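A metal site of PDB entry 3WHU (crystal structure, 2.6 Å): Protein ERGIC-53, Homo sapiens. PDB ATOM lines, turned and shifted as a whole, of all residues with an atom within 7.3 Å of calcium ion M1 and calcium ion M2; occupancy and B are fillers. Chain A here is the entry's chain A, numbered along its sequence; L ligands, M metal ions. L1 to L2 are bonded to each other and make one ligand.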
ATOM      1  N   ASP A  98      14.532 -21.906 -20.936  1.00  0.00           N
ATOM      2  CA  ASP A  98      14.308 -21.170 -22.200  1.00  0.00           C
ATOM      3  C   ASP A  98      13.090 -20.232 -22.114  1.00  0.00           C
ATOM      4  O   ASP A  98      13.050 -19.172 -22.784  1.00  0.00           O
ATOM      5  CB  ASP A  98      14.144 -22.133 -23.387  1.00  0.00           C
ATOM      6  CG  ASP A  98      15.114 -21.830 -24.523  1.00  0.00           C
ATOM      7  OD1 ASP A  98      15.311 -22.744 -25.366  1.00  0.00           O
ATOM      8  OD2 ASP A  98      15.688 -20.704 -24.591  1.00  0.00           O
ATOM      9  N   GLY A  99      12.110 -20.612 -21.302  1.00  0.00           N
ATOM     10  CA  GLY A  99      10.985 -19.752 -20.986  1.00  0.00           C
ATOM     11  C   GLY A  99       9.662 -20.467 -21.068  1.00  0.00           C
ATOM     12  O   GLY A  99       9.576 -21.711 -21.132  1.00  0.00           O
ATOM     13  N   PHE A 115       8.408 -23.518 -27.193  1.00  0.00           N
ATOM     14  CA  PHE A 115       8.424 -23.537 -25.742  1.00  0.00           C
ATOM     15  C   PHE A 115       7.713 -24.786 -25.206  1.00  0.00           C
ATOM     16  O   PHE A 115       6.749 -24.716 -24.421  1.00  0.00           O
ATOM     17  CB  PHE A 115       7.803 -22.254 -25.223  1.00  0.00           C
ATOM     18  CG  PHE A 115       8.663 -21.049 -25.472  1.00  0.00           C
ATOM     19  CD1 PHE A 115       9.406 -20.486 -24.455  1.00  0.00           C
ATOM     20  CD2 PHE A 115       8.748 -20.495 -26.736  1.00  0.00           C
ATOM     21  CE1 PHE A 115      10.217 -19.402 -24.675  1.00  0.00           C
ATOM     22  CE2 PHE A 115       9.555 -19.388 -26.964  1.00  0.00           C
ATOM     23  CZ  PHE A 115      10.293 -18.844 -25.936  1.00  0.00           C
ATOM     24  N   ASP A 129      10.053 -15.093 -22.601  1.00  0.00           N
ATOM     25  CA  ASP A 129      11.276 -15.574 -23.236  1.00  0.00           C
ATOM     26  C   ASP A 129      12.504 -15.135 -22.454  1.00  0.00           C
ATOM     27  O   ASP A 129      12.906 -13.983 -22.474  1.00  0.00           O
ATOM     28  CB  ASP A 129      11.326 -15.072 -24.670  1.00  0.00           C
ATOM     29  CG  ASP A 129      12.366 -15.768 -25.502  1.00  0.00           C
ATOM     30  OD1 ASP A 129      13.382 -16.255 -24.940  1.00  0.00           O
ATOM     31  OD2 ASP A 129      12.190 -15.817 -26.751  1.00  0.00           O
ATOM     32  N   SER A 130      13.100 -16.096 -21.757  1.00  0.00           N
ATOM     33  CA  SER A 130      14.190 -15.825 -20.846  1.00  0.00           C
ATOM     34  C   SER A 130      15.466 -15.607 -21.630  1.00  0.00           C
ATOM     35  O   SER A 130      16.396 -14.946 -21.153  1.00  0.00           O
ATOM     36  CB  SER A 130      14.379 -17.006 -19.883  1.00  0.00           C
ATOM     37  OG  SER A 130      13.161 -17.669 -19.570  1.00  0.00           O
ATOM     38  N   PHE A 131      15.523 -16.216 -22.821  1.00  0.00           N
ATOM     39  CA  PHE A 131      16.776 -16.338 -23.561  1.00  0.00           C
ATOM     40  C   PHE A 131      16.865 -15.501 -24.846  1.00  0.00           C
ATOM     41  O   PHE A 131      16.118 -15.707 -25.805  1.00  0.00           O
ATOM     42  CB  PHE A 131      17.115 -17.806 -23.851  1.00  0.00           C
ATOM     43  CG  PHE A 131      18.569 -18.003 -24.209  1.00  0.00           C
ATOM     44  CD1 PHE A 131      19.578 -17.559 -23.352  1.00  0.00           C
ATOM     45  CD2 PHE A 131      18.931 -18.578 -25.418  1.00  0.00           C
ATOM     46  CE1 PHE A 131      20.907 -17.710 -23.690  1.00  0.00           C
ATOM     47  CE2 PHE A 131      20.273 -18.715 -25.771  1.00  0.00           C
ATOM     48  CZ  PHE A 131      21.255 -18.288 -24.899  1.00  0.00           C
ATOM     49  N   ASP A 132      17.836 -14.588 -24.821  1.00  0.00           N
ATOM     50  CA  ASP A 132      18.132 -13.696 -25.939  1.00  0.00           C
ATOM     51  C   ASP A 132      18.781 -14.458 -27.137  1.00  0.00           C
ATOM     52  O   ASP A 132      19.999 -14.390 -27.332  1.00  0.00           O
ATOM     53  CB  ASP A 132      19.060 -12.572 -25.415  1.00  0.00           C
ATOM     54  CG  ASP A 132      19.222 -11.418 -26.383  1.00  0.00           C
ATOM     55  OD1 ASP A 132      18.229 -11.031 -27.045  1.00  0.00           O
ATOM     56  OD2 ASP A 132      20.356 -10.890 -26.465  1.00  0.00           O
ATOM     57  N   ASN A 133      17.980 -15.174 -27.925  1.00  0.00           N
ATOM     58  CA  ASN A 133      18.492 -16.039 -29.010  1.00  0.00           C
ATOM     59  C   ASN A 133      19.032 -15.305 -30.265  1.00  0.00           C
ATOM     60  O   ASN A 133      19.891 -15.825 -30.978  1.00  0.00           O
ATOM     61  CB  ASN A 133      17.423 -17.032 -29.488  1.00  0.00           C
ATOM     62  CG  ASN A 133      16.921 -17.940 -28.373  1.00  0.00           C
ATOM     63  OD1 ASN A 133      16.541 -17.467 -27.297  1.00  0.00           O
ATOM     64  ND2 ASN A 133      16.876 -19.245 -28.645  1.00  0.00           N
ATOM     65  N   ASP A 134      18.494 -14.124 -30.541  1.00  0.00           N
ATOM     66  CA  ASP A 134      18.954 -13.295 -31.658  1.00  0.00           C
ATOM     67  C   ASP A 134      19.737 -12.098 -31.106  1.00  0.00           C
ATOM     68  O   ASP A 134      19.497 -10.948 -31.495  1.00  0.00           O
ATOM     69  CB  ASP A 134      17.772 -12.854 -32.546  1.00  0.00           C
ATOM     70  CG  ASP A 134      16.646 -12.157 -31.766  1.00  0.00           C
ATOM     71  OD1 ASP A 134      16.934 -11.469 -30.762  1.00  0.00           O
ATOM     72  OD2 ASP A 134      15.475 -12.288 -32.150  1.00  0.00           O
ATOM     73  N   GLY A 135      20.656 -12.377 -30.176  1.00  0.00           N
ATOM     74  CA  GLY A 135      21.684 -11.421 -29.745  1.00  0.00           C
ATOM     75  C   GLY A 135      21.349  -9.939 -29.642  1.00  0.00           C
ATOM     76  O   GLY A 135      22.255  -9.127 -29.670  1.00  0.00           O
ATOM     77  N   LYS A 136      20.069  -9.596 -29.492  1.00  0.00           N
ATOM     78  CA  LYS A 136      19.621  -8.188 -29.468  1.00  0.00           C
ATOM     79  C   LYS A 136      19.607  -7.542 -28.071  1.00  0.00           C
ATOM     80  O   LYS A 136      19.071  -6.452 -27.932  1.00  0.00           O
ATOM     81  CB  LYS A 136      18.207  -8.058 -30.086  1.00  0.00           C
ATOM     82  CG  LYS A 136      18.141  -7.913 -31.602  1.00  0.00           C
ATOM     83  CD  LYS A 136      18.495  -6.503 -32.061  1.00  0.00           C
ATOM     84  CE  LYS A 136      18.537  -6.396 -33.590  1.00  0.00           C
ATOM     85  NZ  LYS A 136      19.305  -5.219 -34.109  1.00  0.00           N
ATOM     86  N   LYS A 137      20.166  -8.178 -27.040  1.00  0.00           N
ATOM     87  CA  LYS A 137      20.083  -7.622 -25.662  1.00  0.00           C
ATOM     88  C   LYS A 137      18.659  -7.095 -25.295  1.00  0.00           C
ATOM     89  O   LYS A 137      18.504  -6.065 -24.620  1.00  0.00           O
ATOM     90  CB  LYS A 137      21.117  -6.504 -25.474  1.00  0.00           C
ATOM     91  CG  LYS A 137      22.538  -6.807 -25.941  1.00  0.00           C
ATOM     92  CD  LYS A 137      23.391  -5.541 -25.888  1.00  0.00           C
ATOM     93  CE  LYS A 137      24.641  -5.627 -26.750  1.00  0.00           C
ATOM     94  NZ  LYS A 137      25.804  -6.199 -26.040  1.00  0.00           N
ATOM     95  N   ASN A 138      17.638  -7.820 -25.735  1.00  0.00           N
ATOM     96  CA  ASN A 138      16.239  -7.417 -25.592  1.00  0.00           C
ATOM     97  C   ASN A 138      15.392  -8.394 -24.739  1.00  0.00           C
ATOM     98  O   ASN A 138      14.159  -8.404 -24.846  1.00  0.00           O
ATOM     99  CB  ASN A 138      15.586  -7.278 -26.993  1.00  0.00           C
ATOM    100  CG  ASN A 138      15.734  -8.543 -27.834  1.00  0.00           C
ATOM    101  OD1 ASN A 138      16.658  -9.357 -27.618  1.00  0.00           O
ATOM    102  ND2 ASN A 138      14.843  -8.717 -28.794  1.00  0.00           N
ATOM    103  N   ASN A 139      16.079  -9.210 -23.910  1.00  0.00           N
ATOM    104  CA  ASN A 139      15.439 -10.277 -23.116  1.00  0.00           C
ATOM    105  C   ASN A 139      15.813 -10.181 -21.632  1.00  0.00           C
ATOM    106  O   ASN A 139      16.854  -9.616 -21.308  1.00  0.00           O
ATOM    107  CB  ASN A 139      15.836 -11.662 -23.661  1.00  0.00           C
ATOM    108  CG  ASN A 139      15.049 -12.061 -24.902  1.00  0.00           C
ATOM    109  OD1 ASN A 139      14.719 -11.224 -25.751  1.00  0.00           O
ATOM    110  ND2 ASN A 139      14.756 -13.344 -25.022  1.00  0.00           N
ATOM    111  N   ALA A 141      11.671 -11.264 -22.104  1.00  0.00           N
ATOM    112  CA  ALA A 141      10.688 -10.522 -22.883  1.00  0.00           C
ATOM    113  C   ALA A 141       9.387 -11.255 -23.103  1.00  0.00           C
ATOM    114  O   ALA A 141       9.366 -12.474 -23.292  1.00  0.00           O
ATOM    115  CB  ALA A 141      11.281 -10.165 -24.226  1.00  0.00           C
ATOM    116  N   TYR A 153       7.343 -20.869 -35.743  1.00  0.00           N
ATOM    117  CA  TYR A 153       7.889 -19.950 -34.736  1.00  0.00           C
ATOM    118  C   TYR A 153       9.421 -19.800 -34.879  1.00  0.00           C
ATOM    119  O   TYR A 153      10.158 -20.800 -34.900  1.00  0.00           O
ATOM    120  CB  TYR A 153       7.486 -20.342 -33.288  1.00  0.00           C
ATOM    121  CG  TYR A 153       8.368 -19.677 -32.274  1.00  0.00           C
ATOM    122  CD1 TYR A 153       8.338 -18.296 -32.113  1.00  0.00           C
ATOM    123  CD2 TYR A 153       9.279 -20.408 -31.530  1.00  0.00           C
ATOM    124  CE1 TYR A 153       9.179 -17.661 -31.202  1.00  0.00           C
ATOM    125  CE2 TYR A 153      10.123 -19.790 -30.619  1.00  0.00           C
ATOM    126  CZ  TYR A 153      10.071 -18.408 -30.455  1.00  0.00           C
ATOM    127  OH  TYR A 153      10.923 -17.795 -29.549  1.00  0.00           O
ATOM    128  N   ASP A 154       9.878 -18.549 -34.970  1.00  0.00           N
ATOM    129  CA  ASP A 154      11.265 -18.283 -35.287  1.00  0.00           C
ATOM    130  C   ASP A 154      12.088 -18.342 -34.031  1.00  0.00           C
ATOM    131  O   ASP A 154      12.560 -17.315 -33.532  1.00  0.00           O
ATOM    132  CB  ASP A 154      11.425 -16.937 -36.007  1.00  0.00           C
ATOM    133  CG  ASP A 154      12.639 -16.930 -36.947  1.00  0.00           C
ATOM    134  OD1 ASP A 154      13.744 -17.369 -36.532  1.00  0.00           O
ATOM    135  OD2 ASP A 154      12.488 -16.486 -38.094  1.00  0.00           O
ATOM    136  N   HIS A 155      12.280 -19.560 -33.538  1.00  0.00           N
ATOM    137  CA  HIS A 155      12.952 -19.777 -32.268  1.00  0.00           C
ATOM    138  C   HIS A 155      14.193 -18.937 -32.163  1.00  0.00           C
ATOM    139  O   HIS A 155      14.293 -18.113 -31.266  1.00  0.00           O
ATOM    140  CB  HIS A 155      13.301 -21.246 -32.019  1.00  0.00           C
ATOM    141  CG  HIS A 155      13.672 -21.538 -30.601  1.00  0.00           C
ATOM    142  ND1 HIS A 155      12.782 -22.072 -29.686  1.00  0.00           N
ATOM    143  CD2 HIS A 155      14.823 -21.319 -29.918  1.00  0.00           C
ATOM    144  CE1 HIS A 155      13.383 -22.195 -28.516  1.00  0.00           C
ATOM    145  NE2 HIS A 155      14.620 -21.748 -28.628  1.00  0.00           N
ATOM    146  N   GLN A 156      15.114 -19.131 -33.107  1.00  0.00           N
ATOM    147  CA  GLN A 156      16.408 -18.439 -33.087  1.00  0.00           C
ATOM    148  C   GLN A 156      16.267 -16.926 -33.129  1.00  0.00           C
ATOM    149  O   GLN A 156      17.159 -16.214 -32.660  1.00  0.00           O
ATOM    150  CB  GLN A 156      17.304 -18.926 -34.223  1.00  0.00           C
ATOM    151  CG  GLN A 156      18.022 -20.226 -33.902  1.00  0.00           C
ATOM    152  CD  GLN A 156      17.813 -21.274 -34.985  1.00  0.00           C
ATOM    153  OE1 GLN A 156      16.670 -21.648 -35.274  1.00  0.00           O
ATOM    154  NE2 GLN A 156      18.904 -21.751 -35.592  1.00  0.00           N
ATOM    155  N   ASN A 157      15.158 -16.439 -33.682  1.00  0.00           N
ATOM    156  CA  ASN A 157      14.877 -15.000 -33.676  1.00  0.00           C
ATOM    157  C   ASN A 157      13.771 -14.553 -32.707  1.00  0.00           C
ATOM    158  O   ASN A 157      13.186 -13.481 -32.908  1.00  0.00           O
ATOM    159  CB  ASN A 157      14.573 -14.490 -35.093  1.00  0.00           C
ATOM    160  CG  ASN A 157      15.821 -14.341 -35.936  1.00  0.00           C
ATOM    161  OD1 ASN A 157      16.682 -13.510 -35.639  1.00  0.00           O
ATOM    162  ND2 ASN A 157      15.931 -15.141 -36.985  1.00  0.00           N
ATOM    163  N   ASP A 158      13.508 -15.338 -31.664  1.00  0.00           N
ATOM    164  CA  ASP A 158      12.585 -14.922 -30.611  1.00  0.00           C
ATOM    165  C   ASP A 158      11.320 -14.323 -31.229  1.00  0.00           C
ATOM    166  O   ASP A 158      10.852 -13.268 -30.802  1.00  0.00           O
ATOM    167  CB  ASP A 158      13.260 -13.871 -29.708  1.00  0.00           C
ATOM    168  CG  ASP A 158      14.422 -14.456 -28.884  1.00  0.00           C
ATOM    169  OD1 ASP A 158      14.356 -15.658 -28.539  1.00  0.00           O
ATOM    170  OD2 ASP A 158      15.385 -13.711 -28.560  1.00  0.00           O
ATOM    171  N   GLY A 159      10.806 -14.989 -32.268  1.00  0.00           N
ATOM    172  CA  GLY A 159       9.692 -14.501 -33.092  1.00  0.00           C
ATOM    173  C   GLY A 159       9.565 -13.007 -33.419  1.00  0.00           C
ATOM    174  O   GLY A 159       8.470 -12.560 -33.769  1.00  0.00           O
ATOM    175  N   ALA A 160      10.655 -12.236 -33.348  1.00  0.00           N
ATOM    176  CA  ALA A 160      10.558 -10.768 -33.377  1.00  0.00           C
ATOM    177  C   ALA A 160       9.742 -10.262 -34.574  1.00  0.00           C
ATOM    178  O   ALA A 160       8.951  -9.343 -34.445  1.00  0.00           O
ATOM    179  CB  ALA A 160      11.937 -10.119 -33.310  1.00  0.00           C
ATOM    180  N   GLN A 168       8.954  -5.805 -22.555  1.00  0.00           N
ATOM    181  CA  GLN A 168      10.181  -6.276 -21.952  1.00  0.00           C
ATOM    182  C   GLN A 168      10.175  -6.147 -20.456  1.00  0.00           C
ATOM    183  O   GLN A 168      10.627  -5.142 -19.921  1.00  0.00           O
ATOM    184  CB  GLN A 168      11.379  -5.498 -22.515  1.00  0.00           C
ATOM    185  CG  GLN A 168      12.041  -6.140 -23.739  1.00  0.00           C
ATOM    186  CD  GLN A 168      13.440  -5.596 -24.032  1.00  0.00           C
ATOM    187  OE1 GLN A 168      13.778  -5.377 -25.190  1.00  0.00           O
ATOM    188  NE2 GLN A 168      14.244  -5.404 -22.989  1.00  0.00           N
HETATM  189  C1  LIG L   1      21.085 -23.701 -26.889  1.00  0.00           C
HETATM  190  C2  LIG L   1      19.916 -23.881 -27.886  1.00  0.00           C
HETATM  191  C3  LIG L   1      18.892 -22.764 -27.926  1.00  0.00           C
HETATM  192  C4  LIG L   1      18.539 -22.348 -26.499  1.00  0.00           C
HETATM  193  C5  LIG L   1      19.754 -22.129 -25.601  1.00  0.00           C
HETATM  194  C6  LIG L   1      19.328 -22.020 -24.139  1.00  0.00           C
HETATM  195  O1  LIG L   1      22.098 -22.871 -27.408  1.00  0.00           O
HETATM  196  O2  LIG L   1      19.122 -25.026 -27.614  1.00  0.00           O
HETATM  197  O3  LIG L   1      17.740 -23.284 -28.588  1.00  0.00           O
HETATM  198  O4  LIG L   1      17.782 -21.157 -26.549  1.00  0.00           O
HETATM  199  O5  LIG L   1      20.700 -23.166 -25.632  1.00  0.00           O
HETATM  200  O6  LIG L   1      18.838 -23.286 -23.686  1.00  0.00           O
HETATM  201  C1  LG2 L   2      19.349 -25.993 -28.620  1.00  0.00           C
HETATM  202  C2  LG2 L   2      18.451 -27.245 -28.499  1.00  0.00           C
HETATM  203  C3  LG2 L   2      18.879 -28.136 -27.304  1.00  0.00           C
HETATM  204  C4  LG2 L   2      20.382 -28.432 -27.478  1.00  0.00           C
HETATM  205  C5  LG2 L   2      21.106 -27.067 -27.366  1.00  0.00           C
HETATM  206  C6  LG2 L   2      22.642 -27.141 -27.250  1.00  0.00           C
HETATM  207  O1  LG2 L   2      18.486 -27.953 -29.757  1.00  0.00           O
HETATM  208  O2  LG2 L   2      18.133 -29.354 -27.161  1.00  0.00           O
HETATM  209  O3  LG2 L   2      20.803 -29.422 -26.550  1.00  0.00           O
HETATM  210  O4  LG2 L   2      20.731 -26.278 -28.491  1.00  0.00           O
HETATM  211  O5  LG2 L   2      23.156 -27.681 -28.461  1.00  0.00           O
HETATM  212 CA    CA M   1      15.345 -11.525 -28.749  1.00  0.00          CA
HETATM  213 CA    CA M   2      14.384 -17.302 -27.065  1.00  0.00          CA
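The side-chain amide nitrogen (ND2) of Asn 133 is in hydrogen-bond range of an oxygen (O4) of LIG L1, at 3.0 Å. An oxygen (O3) of LIG L1 lies within hydrogen-bond range of a ring nitrogen (NE2) of His 155 (3.5 Å). An oxygen (O4) of LIG L1 sits at hydrogen-bond distance from the side-chain carboxylate (OD2) of Asp 98 (2.9 Å).
Four residues have an atom within 4 Å of calcium ion M2: Asp 129, Phe 131, Asn 133 and Asp 158.
The side-chain carboxylate of Asp 134 lies close to the backbone carbonyl oxygen of Asn 157 (2.7 Å). The backbone NH (N) of Asp 134 sits at hydrogen-bond distance from the backbone carbonyl oxygen (O) of Gln 156, at 3.3 Å. O of Asp 129 sits at hydrogen-bond distance from ND2 of Asn 139 (3.2 Å). The backbone NH of Asp 129 sits at hydrogen-bond distance from the backbone carbonyl oxygen of Ala 141 (2.8 Å). OD1 of Asn 139 sits close to OD1 of Asn 138, 3.3 Å away. The backbone carbonyl oxygen of Asn 138 lies close to the side-chain amide oxygen of Gln 168 (3.1 Å). The backbone NH (N) of Lys 136 lies within hydrogen-bond range of the side-chain carboxylate (OD2) of Asp 132 (3.3 Å). OD2 of Asp 132 sits at hydrogen-bond distance from N of Lys 137, at 2.8 Å.
Residues that only touch calcium ion M1: Asp 132. The nearest printed residue that does not touch calcium ion M1 is Asn 133 (4.6 Å).
Calcium ion M1 is bound by OD2 of Asp 158 (2.2 Å), OD1 of Asp 134 (2.6 Å), OD1 of Asn 138 (2.8 Å) and ND2 of Asn 138 (2.9 Å). Calcium ion M1 has four donor atoms within binding distance. Slightly farther from calcium ion M1 lies OD1 of Asn 139 (3.1 Å).
Calcium ion M2 is bound by the side-chain amide oxygen (OD1) of Asn 133 (2.2 Å), the side-chain carboxylate (OD1) of Asp 158 (2.2 Å), the side-chain carboxylate (OD1) of Asp 129 (2.6 Å), the side-chain carboxylate (OD2) of Asp 129 (2.7 Å) and the backbone carbonyl oxygen (O) of Phe 131 (2.7 Å).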
